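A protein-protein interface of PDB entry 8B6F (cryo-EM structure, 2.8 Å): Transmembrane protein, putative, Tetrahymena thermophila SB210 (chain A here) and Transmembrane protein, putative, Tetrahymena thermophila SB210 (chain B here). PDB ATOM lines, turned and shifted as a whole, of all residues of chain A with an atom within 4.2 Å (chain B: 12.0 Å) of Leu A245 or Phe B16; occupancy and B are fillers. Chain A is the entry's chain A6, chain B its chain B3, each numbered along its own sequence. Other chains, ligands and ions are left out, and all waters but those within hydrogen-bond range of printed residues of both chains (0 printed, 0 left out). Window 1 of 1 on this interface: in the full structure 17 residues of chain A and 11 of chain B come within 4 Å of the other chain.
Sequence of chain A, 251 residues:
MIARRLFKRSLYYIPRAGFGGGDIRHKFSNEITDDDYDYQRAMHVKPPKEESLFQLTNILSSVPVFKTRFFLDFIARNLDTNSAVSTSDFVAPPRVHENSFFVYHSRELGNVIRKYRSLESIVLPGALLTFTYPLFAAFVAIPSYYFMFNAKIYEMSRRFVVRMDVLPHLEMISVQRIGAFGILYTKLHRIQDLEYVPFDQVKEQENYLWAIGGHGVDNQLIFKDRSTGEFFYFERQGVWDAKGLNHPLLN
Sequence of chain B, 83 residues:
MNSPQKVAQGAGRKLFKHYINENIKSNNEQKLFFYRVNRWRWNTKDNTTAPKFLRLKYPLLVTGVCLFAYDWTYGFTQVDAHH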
ATOM      1  N   VAL A 103      -0.069  32.940  19.623  1.00  0.00           N
ATOM      2  CA  VAL A 103      -0.092  32.910  18.164  1.00  0.00           C
ATOM      3  C   VAL A 103      -1.281  33.710  17.646  1.00  0.00           C
ATOM      4  O   VAL A 103      -1.124  34.589  16.793  1.00  0.00           O
ATOM      5  CB  VAL A 103      -0.140  31.460  17.647  1.00  0.00           C
ATOM      6  CG1 VAL A 103      -0.225  31.430  16.128  1.00  0.00           C
ATOM      7  CG2 VAL A 103       1.073  30.686  18.130  1.00  0.00           C
ATOM      8  N   MET A 164      -5.164  31.491  21.257  1.00  0.00           N
ATOM      9  CA  MET A 164      -4.371  30.300  20.979  1.00  0.00           C
ATOM     10  C   MET A 164      -2.921  30.592  21.324  1.00  0.00           C
ATOM     11  O   MET A 164      -2.343  31.554  20.812  1.00  0.00           O
ATOM     12  CB  MET A 164      -4.502  29.878  19.514  1.00  0.00           C
ATOM     13  CG  MET A 164      -3.869  28.530  19.216  1.00  0.00           C
ATOM     14  SD  MET A 164      -4.170  27.948  17.536  1.00  0.00           S
ATOM     15  CE  MET A 164      -3.307  29.194  16.584  1.00  0.00           C
ATOM     16  N   ILE A 173      -0.827  22.969  22.037  1.00  0.00           N
ATOM     17  CA  ILE A 173      -1.459  24.263  21.813  1.00  0.00           C
ATOM     18  C   ILE A 173      -2.584  24.417  22.825  1.00  0.00           C
ATOM     19  O   ILE A 173      -3.446  23.538  22.942  1.00  0.00           O
ATOM     20  CB  ILE A 173      -1.985  24.411  20.373  1.00  0.00           C
ATOM     21  CG1 ILE A 173      -0.881  24.019  19.386  1.00  0.00           C
ATOM     22  CG2 ILE A 173      -2.475  25.827  20.129  1.00  0.00           C
ATOM     23  CD1 ILE A 173      -1.140  24.415  17.946  1.00  0.00           C
ATOM     24  N   PHE A 223      -9.636  24.222  11.397  1.00  0.00           N
ATOM     25  CA  PHE A 223      -8.829  23.096  11.838  1.00  0.00           C
ATOM     26  C   PHE A 223      -9.637  22.272  12.831  1.00  0.00           C
ATOM     27  O   PHE A 223     -10.621  22.746  13.406  1.00  0.00           O
ATOM     28  CB  PHE A 223      -7.517  23.552  12.485  1.00  0.00           C
ATOM     29  CG  PHE A 223      -6.504  24.068  11.506  1.00  0.00           C
ATOM     30  CD1 PHE A 223      -6.581  25.364  11.025  1.00  0.00           C
ATOM     31  CD2 PHE A 223      -5.466  23.258  11.074  1.00  0.00           C
ATOM     32  CE1 PHE A 223      -5.646  25.841  10.128  1.00  0.00           C
ATOM     33  CE2 PHE A 223      -4.528  23.728  10.177  1.00  0.00           C
ATOM     34  CZ  PHE A 223      -4.618  25.021   9.703  1.00  0.00           C
ATOM     35  N   PHE A 234     -11.522  30.524  13.815  1.00  0.00           N
ATOM     36  CA  PHE A 234     -10.706  31.710  14.038  1.00  0.00           C
ATOM     37  C   PHE A 234     -11.416  32.924  13.456  1.00  0.00           C
ATOM     38  O   PHE A 234     -11.931  32.868  12.335  1.00  0.00           O
ATOM     39  CB  PHE A 234      -9.321  31.548  13.408  1.00  0.00           C
ATOM     40  CG  PHE A 234      -8.573  30.345  13.899  1.00  0.00           C
ATOM     41  CD1 PHE A 234      -7.970  30.350  15.144  1.00  0.00           C
ATOM     42  CD2 PHE A 234      -8.468  29.211  13.113  1.00  0.00           C
ATOM     43  CE1 PHE A 234      -7.281  29.247  15.598  1.00  0.00           C
ATOM     44  CE2 PHE A 234      -7.779  28.102  13.564  1.00  0.00           C
ATOM     45  CZ  PHE A 234      -7.185  28.121  14.808  1.00  0.00           C
ATOM     46  N   TRP A 240      -2.921  37.806  14.322  1.00  0.00           N
ATOM     47  CA  TRP A 240      -1.976  36.703  14.298  1.00  0.00           C
ATOM     48  C   TRP A 240      -0.569  37.239  14.518  1.00  0.00           C
ATOM     49  O   TRP A 240      -0.263  38.384  14.175  1.00  0.00           O
ATOM     50  CB  TRP A 240      -2.034  35.943  12.969  1.00  0.00           C
ATOM     51  CG  TRP A 240      -3.302  35.181  12.762  1.00  0.00           C
ATOM     52  CD1 TRP A 240      -4.479  35.667  12.276  1.00  0.00           C
ATOM     53  CD2 TRP A 240      -3.521  33.793  13.031  1.00  0.00           C
ATOM     54  NE1 TRP A 240      -5.419  34.668  12.227  1.00  0.00           N
ATOM     55  CE2 TRP A 240      -4.855  33.507  12.686  1.00  0.00           C
ATOM     56  CE3 TRP A 240      -2.719  32.764  13.532  1.00  0.00           C
ATOM     57  CZ2 TRP A 240      -5.406  32.235  12.824  1.00  0.00           C
ATOM     58  CZ3 TRP A 240      -3.265  31.502  13.670  1.00  0.00           C
ATOM     59  CH2 TRP A 240      -4.598  31.248  13.318  1.00  0.00           C
ATOM     60  N   ASP A 241       0.285  36.405  15.099  1.00  0.00           N
ATOM     61  CA  ASP A 241       1.667  36.766  15.375  1.00  0.00           C
ATOM     62  C   ASP A 241       2.576  36.147  14.324  1.00  0.00           C
ATOM     63  O   ASP A 241       2.549  34.931  14.112  1.00  0.00           O
ATOM     64  CB  ASP A 241       2.080  36.305  16.773  1.00  0.00           C
ATOM     65  CG  ASP A 241       3.489  36.729  17.134  1.00  0.00           C
ATOM     66  OD1 ASP A 241       3.750  37.949  17.187  1.00  0.00           O
ATOM     67  OD2 ASP A 241       4.335  35.843  17.367  1.00  0.00           O
ATOM     68  N   ALA A 242       3.379  36.987  13.668  1.00  0.00           N
ATOM     69  CA  ALA A 242       4.290  36.487  12.645  1.00  0.00           C
ATOM     70  C   ALA A 242       5.291  35.503  13.235  1.00  0.00           C
ATOM     71  O   ALA A 242       5.549  34.443  12.655  1.00  0.00           O
ATOM     72  CB  ALA A 242       5.018  37.652  11.977  1.00  0.00           C
ATOM     73  N   LYS A 243       5.868  35.840  14.390  1.00  0.00           N
ATOM     74  CA  LYS A 243       6.822  34.940  15.028  1.00  0.00           C
ATOM     75  C   LYS A 243       6.157  33.626  15.420  1.00  0.00           C
ATOM     76  O   LYS A 243       6.731  32.548  15.224  1.00  0.00           O
ATOM     77  CB  LYS A 243       7.441  35.616  16.249  1.00  0.00           C
ATOM     78  CG  LYS A 243       8.524  34.791  16.930  1.00  0.00           C
ATOM     79  CD  LYS A 243       9.038  35.464  18.196  1.00  0.00           C
ATOM     80  CE  LYS A 243       9.678  36.815  17.906  1.00  0.00           C
ATOM     81  NZ  LYS A 243      10.751  36.727  16.876  1.00  0.00           N
ATOM     82  N   GLY A 244       4.947  33.694  15.975  1.00  0.00           N
ATOM     83  CA  GLY A 244       4.246  32.475  16.344  1.00  0.00           C
ATOM     84  C   GLY A 244       3.952  31.590  15.149  1.00  0.00           C
ATOM     85  O   GLY A 244       4.095  30.368  15.219  1.00  0.00           O
ATOM     86  N   LEU A 245       3.539  32.193  14.034  1.00  0.00           N
ATOM     87  CA  LEU A 245       3.278  31.417  12.827  1.00  0.00           C
ATOM     88  C   LEU A 245       4.559  30.809  12.271  1.00  0.00           C
ATOM     89  O   LEU A 245       4.550  29.677  11.772  1.00  0.00           O
ATOM     90  CB  LEU A 245       2.604  32.296  11.774  1.00  0.00           C
ATOM     91  CG  LEU A 245       1.155  32.700  12.054  1.00  0.00           C
ATOM     92  CD1 LEU A 245       0.668  33.686  11.008  1.00  0.00           C
ATOM     93  CD2 LEU A 245       0.253  31.476  12.087  1.00  0.00           C
ATOM     94  N   ASN A 246       5.668  31.541  12.344  1.00  0.00           N
ATOM     95  CA  ASN A 246       6.930  31.079  11.782  1.00  0.00           C
ATOM     96  C   ASN A 246       7.711  30.174  12.726  1.00  0.00           C
ATOM     97  O   ASN A 246       8.769  29.672  12.334  1.00  0.00           O
ATOM     98  CB  ASN A 246       7.797  32.277  11.394  1.00  0.00           C
ATOM     99  CG  ASN A 246       7.108  33.197  10.411  1.00  0.00           C
ATOM    100  OD1 ASN A 246       5.886  33.180  10.281  1.00  0.00           O
ATOM    101  ND2 ASN A 246       7.893  34.007   9.710  1.00  0.00           N
ATOM    102  N   HIS A 247       7.231  29.955  13.943  1.00  0.00           N
ATOM    103  CA  HIS A 247       7.936  29.071  14.857  1.00  0.00           C
ATOM    104  C   HIS A 247       8.027  27.672  14.251  1.00  0.00           C
ATOM    105  O   HIS A 247       7.052  27.184  13.669  1.00  0.00           O
ATOM    106  CB  HIS A 247       7.217  29.013  16.206  1.00  0.00           C
ATOM    107  CG  HIS A 247       8.059  28.461  17.313  1.00  0.00           C
ATOM    108  ND1 HIS A 247       9.026  29.206  17.955  1.00  0.00           N
ATOM    109  CD2 HIS A 247       8.087  27.236  17.888  1.00  0.00           C
ATOM    110  CE1 HIS A 247       9.609  28.465  18.879  1.00  0.00           C
ATOM    111  NE2 HIS A 247       9.058  27.265  18.859  1.00  0.00           N
ATOM    112  N   LEU A 250       5.111  24.917  14.591  1.00  0.00           N
ATOM    113  CA  LEU A 250       3.901  25.042  13.793  1.00  0.00           C
ATOM    114  C   LEU A 250       4.171  24.993  12.295  1.00  0.00           C
ATOM    115  O   LEU A 250       3.248  25.215  11.506  1.00  0.00           O
ATOM    116  CB  LEU A 250       3.172  26.342  14.141  1.00  0.00           C
ATOM    117  CG  LEU A 250       2.611  26.443  15.560  1.00  0.00           C
ATOM    118  CD1 LEU A 250       1.997  27.811  15.779  1.00  0.00           C
ATOM    119  CD2 LEU A 250       1.591  25.351  15.833  1.00  0.00           C
ATOM    120  N   ASN A 251       5.404  24.715  11.888  1.00  0.00           N
ATOM    121  CA  ASN A 251       5.740  24.619  10.474  1.00  0.00           C
ATOM    122  C   ASN A 251       6.454  23.306  10.183  1.00  0.00           C
ATOM    123  O   ASN A 251       6.951  22.647  11.096  1.00  0.00           O
ATOM    124  CB  ASN A 251       6.615  25.800  10.052  1.00  0.00           C
ATOM    125  CG  ASN A 251       5.947  27.132  10.304  1.00  0.00           C
ATOM    126  OD1 ASN A 251       5.202  27.634   9.466  1.00  0.00           O
ATOM    127  ND2 ASN A 251       6.205  27.712  11.469  1.00  0.00           N
ATOM    128  OXT ASN A 251       6.547  22.871   9.035  1.00  0.00           O
ATOM    129  N   ALA B  11       8.074  20.759  11.438  1.00  0.00           N
ATOM    130  CA  ALA B  11       8.782  19.603  10.824  1.00  0.00           C
ATOM    131  C   ALA B  11       8.069  19.148   9.557  1.00  0.00           C
ATOM    132  O   ALA B  11       7.656  17.993   9.449  1.00  0.00           O
ATOM    133  CB  ALA B  11       8.883  18.459  11.817  1.00  0.00           C
ATOM    134  N   GLY B  12       7.930  20.059   8.600  1.00  0.00           N
ATOM    135  CA  GLY B  12       7.264  19.722   7.351  1.00  0.00           C
ATOM    136  C   GLY B  12       5.812  19.337   7.528  1.00  0.00           C
ATOM    137  O   GLY B  12       5.351  18.366   6.915  1.00  0.00           O
ATOM    138  N   ARG B  13       5.079  20.075   8.357  1.00  0.00           N
ATOM    139  CA  ARG B  13       3.674  19.803   8.629  1.00  0.00           C
ATOM    140  C   ARG B  13       2.838  21.001   8.208  1.00  0.00           C
ATOM    141  O   ARG B  13       3.149  22.140   8.570  1.00  0.00           O
ATOM    142  CB  ARG B  13       3.454  19.493  10.113  1.00  0.00           C
ATOM    143  CG  ARG B  13       4.082  20.510  11.056  1.00  0.00           C
ATOM    144  CD  ARG B  13       3.975  20.070  12.507  1.00  0.00           C
ATOM    145  NE  ARG B  13       4.619  18.783  12.737  1.00  0.00           N
ATOM    146  CZ  ARG B  13       4.797  18.234  13.932  1.00  0.00           C
ATOM    147  NH1 ARG B  13       4.406  18.845  15.038  1.00  0.00           N
ATOM    148  NH2 ARG B  13       5.384  17.044  14.018  1.00  0.00           N
ATOM    149  N   LYS B  14       1.780  20.738   7.444  1.00  0.00           N
ATOM    150  CA  LYS B  14       0.905  21.800   6.965  1.00  0.00           C
ATOM    151  C   LYS B  14       0.024  22.287   8.108  1.00  0.00           C
ATOM    152  O   LYS B  14      -0.725  21.504   8.700  1.00  0.00           O
ATOM    153  CB  LYS B  14       0.057  21.293   5.800  1.00  0.00           C
ATOM    154  CG  LYS B  14       0.883  20.815   4.612  1.00  0.00           C
ATOM    155  CD  LYS B  14       0.011  20.339   3.458  1.00  0.00           C
ATOM    156  CE  LYS B  14      -0.731  19.056   3.803  1.00  0.00           C
ATOM    157  NZ  LYS B  14      -1.501  18.530   2.638  1.00  0.00           N
ATOM    158  N   LEU B  15       0.107  23.577   8.414  1.00  0.00           N
ATOM    159  CA  LEU B  15      -0.552  24.135   9.589  1.00  0.00           C
ATOM    160  C   LEU B  15      -0.944  25.579   9.283  1.00  0.00           C
ATOM    161  O   LEU B  15      -1.005  25.984   8.119  1.00  0.00           O
ATOM    162  CB  LEU B  15       0.357  23.995  10.825  1.00  0.00           C
ATOM    163  CG  LEU B  15       0.512  22.588  11.408  1.00  0.00           C
ATOM    164  CD1 LEU B  15       1.471  22.612  12.582  1.00  0.00           C
ATOM    165  CD2 LEU B  15      -0.828  22.009  11.836  1.00  0.00           C
ATOM    166  N   PHE B  16      -1.213  26.352  10.338  1.00  0.00           N
ATOM    167  CA  PHE B  16      -1.845  27.660  10.190  1.00  0.00           C
ATOM    168  C   PHE B  16      -1.121  28.533   9.173  1.00  0.00           C
ATOM    169  O   PHE B  16      -1.751  29.137   8.299  1.00  0.00           O
ATOM    170  CB  PHE B  16      -1.899  28.354  11.553  1.00  0.00           C
ATOM    171  CG  PHE B  16      -2.515  27.513  12.632  1.00  0.00           C
ATOM    172  CD1 PHE B  16      -3.889  27.362  12.714  1.00  0.00           C
ATOM    173  CD2 PHE B  16      -1.719  26.869  13.564  1.00  0.00           C
ATOM    174  CE1 PHE B  16      -4.455  26.584  13.705  1.00  0.00           C
ATOM    175  CE2 PHE B  16      -2.279  26.091  14.555  1.00  0.00           C
ATOM    176  CZ  PHE B  16      -3.650  25.948  14.626  1.00  0.00           C
ATOM    177  N   LYS B  17       0.206  28.615   9.267  1.00  0.00           N
ATOM    178  CA  LYS B  17       0.950  29.462   8.341  1.00  0.00           C
ATOM    179  C   LYS B  17       0.783  28.974   6.908  1.00  0.00           C
ATOM    180  O   LYS B  17       0.556  29.771   5.991  1.00  0.00           O
ATOM    181  CB  LYS B  17       2.429  29.499   8.721  1.00  0.00           C
ATOM    182  CG  LYS B  17       3.257  30.448   7.861  1.00  0.00           C
ATOM    183  CD  LYS B  17       4.745  30.219   8.055  1.00  0.00           C
ATOM    184  CE  LYS B  17       5.567  31.156   7.185  1.00  0.00           C
ATOM    185  NZ  LYS B  17       7.028  30.887   7.306  1.00  0.00           N
ATOM    186  N   HIS B  18       0.899  27.664   6.695  1.00  0.00           N
ATOM    187  CA  HIS B  18       0.791  27.123   5.345  1.00  0.00           C
ATOM    188  C   HIS B  18      -0.567  27.435   4.732  1.00  0.00           C
ATOM    189  O   HIS B  18      -0.655  27.889   3.587  1.00  0.00           O
ATOM    190  CB  HIS B  18       1.031  25.613   5.381  1.00  0.00           C
ATOM    191  CG  HIS B  18       0.849  24.939   4.057  1.00  0.00           C
ATOM    192  ND1 HIS B  18      -0.366  24.441   3.638  1.00  0.00           N
ATOM    193  CD2 HIS B  18       1.726  24.676   3.061  1.00  0.00           C
ATOM    194  CE1 HIS B  18      -0.229  23.900   2.441  1.00  0.00           C
ATOM    195  NE2 HIS B  18       1.031  24.031   2.067  1.00  0.00           N
ATOM    196  N   TYR B  19      -1.643  27.202   5.484  1.00  0.00           N
ATOM    197  CA  TYR B  19      -2.980  27.411   4.943  1.00  0.00           C
ATOM    198  C   TYR B  19      -3.346  28.887   4.863  1.00  0.00           C
ATOM    199  O   TYR B  19      -4.155  29.272   4.013  1.00  0.00           O
ATOM    200  CB  TYR B  19      -4.001  26.635   5.768  1.00  0.00           C
ATOM    201  CG  TYR B  19      -3.889  25.147   5.544  1.00  0.00           C
ATOM    202  CD1 TYR B  19      -4.366  24.565   4.376  1.00  0.00           C
ATOM    203  CD2 TYR B  19      -3.286  24.329   6.485  1.00  0.00           C
ATOM    204  CE1 TYR B  19      -4.255  23.207   4.160  1.00  0.00           C
ATOM    205  CE2 TYR B  19      -3.171  22.970   6.279  1.00  0.00           C
ATOM    206  CZ  TYR B  19      -3.658  22.416   5.114  1.00  0.00           C
ATOM    207  OH  TYR B  19      -3.544  21.062   4.907  1.00  0.00           O
ATOM    208  N   ILE B  20      -2.766  29.725   5.724  1.00  0.00           N
ATOM    209  CA  ILE B  20      -2.938  31.165   5.566  1.00  0.00           C
ATOM    210  C   ILE B  20      -2.319  31.624   4.255  1.00  0.00           C
ATOM    211  O   ILE B  20      -2.908  32.422   3.518  1.00  0.00           O
ATOM    212  CB  ILE B  20      -2.340  31.911   6.776  1.00  0.00           C
ATOM    213  CG1 ILE B  20      -3.238  31.733   8.001  1.00  0.00           C
ATOM    214  CG2 ILE B  20      -2.140  33.393   6.466  1.00  0.00           C
ATOM    215  CD1 ILE B  20      -2.592  32.154   9.301  1.00  0.00           C
ATOM    216  N   ASN B  21      -1.124  31.122   3.940  1.00  0.00           N
ATOM    217  CA  ASN B  21      -0.506  31.451   2.662  1.00  0.00           C
ATOM    218  C   ASN B  21      -1.346  30.935   1.501  1.00  0.00           C
ATOM    219  O   ASN B  21      -1.493  31.616   0.480  1.00  0.00           O
ATOM    220  CB  ASN B  21       0.906  30.874   2.603  1.00  0.00           C
ATOM    221  CG  ASN B  21       1.838  31.519   3.606  1.00  0.00           C
ATOM    222  OD1 ASN B  21       1.396  32.204   4.527  1.00  0.00           O
ATOM    223  ND2 ASN B  21       3.136  31.301   3.433  1.00  0.00           N
ATOM    224  N   GLU B  22      -1.908  29.733   1.639  1.00  0.00           N
ATOM    225  CA  GLU B  22      -2.770  29.200   0.590  1.00  0.00           C
ATOM    226  C   GLU B  22      -3.988  30.089   0.372  1.00  0.00           C
ATOM    227  O   GLU B  22      -4.361  30.372  -0.773  1.00  0.00           O
ATOM    228  CB  GLU B  22      -3.208  27.780   0.948  1.00  0.00           C
ATOM    229  CG  GLU B  22      -2.092  26.754   0.889  1.00  0.00           C
ATOM    230  CD  GLU B  22      -1.579  26.533  -0.517  1.00  0.00           C
ATOM    231  OE1 GLU B  22      -2.256  26.966  -1.473  1.00  0.00           O
ATOM    232  OE2 GLU B  22      -0.497  25.928  -0.669  1.00  0.00           O
ATOM    233  N   ASN B  23      -4.624  30.536   1.456  1.00  0.00           N
ATOM    234  CA  ASN B  23      -5.787  31.409   1.318  1.00  0.00           C
ATOM    235  C   ASN B  23      -5.403  32.748   0.702  1.00  0.00           C
ATOM    236  O   ASN B  23      -6.150  33.299  -0.114  1.00  0.00           O
ATOM    237  CB  ASN B  23      -6.454  31.608   2.678  1.00  0.00           C
ATOM    238  CG  ASN B  23      -7.021  30.316   3.239  1.00  0.00           C
ATOM    239  OD1 ASN B  23      -6.707  29.231   2.754  1.00  0.00           O
ATOM    240  ND2 ASN B  23      -7.864  30.426   4.259  1.00  0.00           N
ATOM    241  N   ILE B  24      -4.247  33.292   1.085  1.00  0.00           N
ATOM    242  CA  ILE B  24      -3.785  34.548   0.498  1.00  0.00           C
ATOM    243  C   ILE B  24      -3.558  34.378  -0.997  1.00  0.00           C
ATOM    244  O   ILE B  24      -3.926  35.242  -1.801  1.00  0.00           O
ATOM    245  CB  ILE B  24      -2.513  35.038   1.215  1.00  0.00           C
ATOM    246  CG1 ILE B  24      -2.839  35.445   2.652  1.00  0.00           C
ATOM    247  CG2 ILE B  24      -1.884  36.208   0.465  1.00  0.00           C
ATOM    248  CD1 ILE B  24      -1.617  35.662   3.521  1.00  0.00           C
ATOM    249  N   LYS B  25      -2.945  33.262  -1.392  1.00  0.00           N
ATOM    250  CA  LYS B  25      -2.734  32.994  -2.809  1.00  0.00           C
ATOM    251  C   LYS B  25      -4.059  32.868  -3.545  1.00  0.00           C
ATOM    252  O   LYS B  25      -4.222  33.406  -4.647  1.00  0.00           O
ATOM    253  CB  LYS B  25      -1.905  31.721  -2.974  1.00  0.00           C
ATOM    254  CG  LYS B  25      -1.492  31.420  -4.405  1.00  0.00           C
ATOM    255  CD  LYS B  25      -0.984  29.991  -4.544  1.00  0.00           C
ATOM    256  CE  LYS B  25       0.201  29.719  -3.627  1.00  0.00           C
ATOM    257  NZ  LYS B  25       0.719  28.332  -3.790  1.00  0.00           N
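The backbone NH (N) of Gly B12 lies within hydrogen-bond range of the chain-end carboxylate (OXT) of Asn A251, 3.2 Å away.
N of Arg B13 is in hydrogen-bond range of OXT of Asn A251 (3.2 Å).
The chain-end carboxylate (O) of Asn A251 sits close to the backbone NH (N) of Ala B11 (2.2 Å).
O of Lys B17 sits close to OD1 of Asn B21, 3.0 Å away.
O of Tyr B19 lies close to OD1 of Asn B23, at 2.8 Å.
The backbone carbonyl oxygen of Met A164 sits at hydrogen-bond distance from the backbone NH of Val A103 (2.9 Å).
OD1 of Asn A246 lies close to O of Ala A242 (2.7 Å).
The backbone carbonyl oxygen (O) of Leu A245 lies within hydrogen-bond range of the side-chain amide nitrogen (ND2) of Asn A251 (2.6 Å).
O of His A247 lies within hydrogen-bond range of ND2 of Asn A251 (2.4 Å).
Among the printed residues, merely in contact across the chains: Asn A251 with Lys B17, Leu A250 with Leu B15, Phe A234 with Phe B16, Phe A223 with Phe B16, Phe A223 with Tyr B19, Met A164 with Phe B16, Asn A246 with Lys B17, Leu A245 with Lys B17, Phe A223 with Leu B15, Leu A245 with Phe B16, Ile A173 with Phe B16, Leu A245 with Ile B20 and Trp A240 with Phe B16.
No residue of chain B comes within 4 Å of Val A103.
Printed residues of chain B within 4 Å of Trp A240: Phe B16 (3.996 Å).
No residue of chain B comes within 4 Å of Asp A241.
No residue of chain B comes within 4 Å of Ala A242.
No residue of chain B comes within 4 Å of Gly A244.
Of the printed residues of chain B, Leu A245 touches Phe B16 (3.8 Å), Lys B17 (3.7 Å) and Ile B20 (3.99 Å).
Of chain B, only Lys B17 comes within 4 Å of Asn A246.
Leu A250 touches one residue of chain B.
Of chain B, only Ala B11 (2.2 Å), Gly B12 (3.2 Å), Arg B13 (3.2 Å) and Lys B17 (3.0 Å) come within 4 Å of Asn A251.
Of the printed residues of chain A, Ala B11 touches Asn A251 (2.2 Å).
Printed residues of chain A within 4 Å of Leu B15: Phe A223 (3.7 Å) and Leu A250 (3.2 Å).
Of the printed residues of chain A, Phe B16 touches Met A164, Ile A173, Phe A223, Phe A234, Trp A240 and Leu A245.
Of the printed residues of chain A, Lys B17 touches Leu A245, Asn A246 and Asn A251.
The nearest printed residue of chain B that does not touch Leu A245 is His B18 (6.6 Å).
Of the 15 printed residues of chain A, 9 touch a printed residue of chain B.
Hydrophobic or aromatic side chains of chain A within 4 Å of the printed part of chain B: Met A164, Ile A173, Phe A223, Phe A234, Trp A240 and Leu A245.
Printed residues of chain B that touch a printed residue of chain A: Ala B11, Gly B12, Arg B13, Leu B15, Phe B16, Lys B17, Tyr B19 and Ile B20.
Hydrophobic or aromatic side chains of chain B within 4 Å of the printed part of chain A: Leu B15, Phe B16, Tyr B19 and Ile B20.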
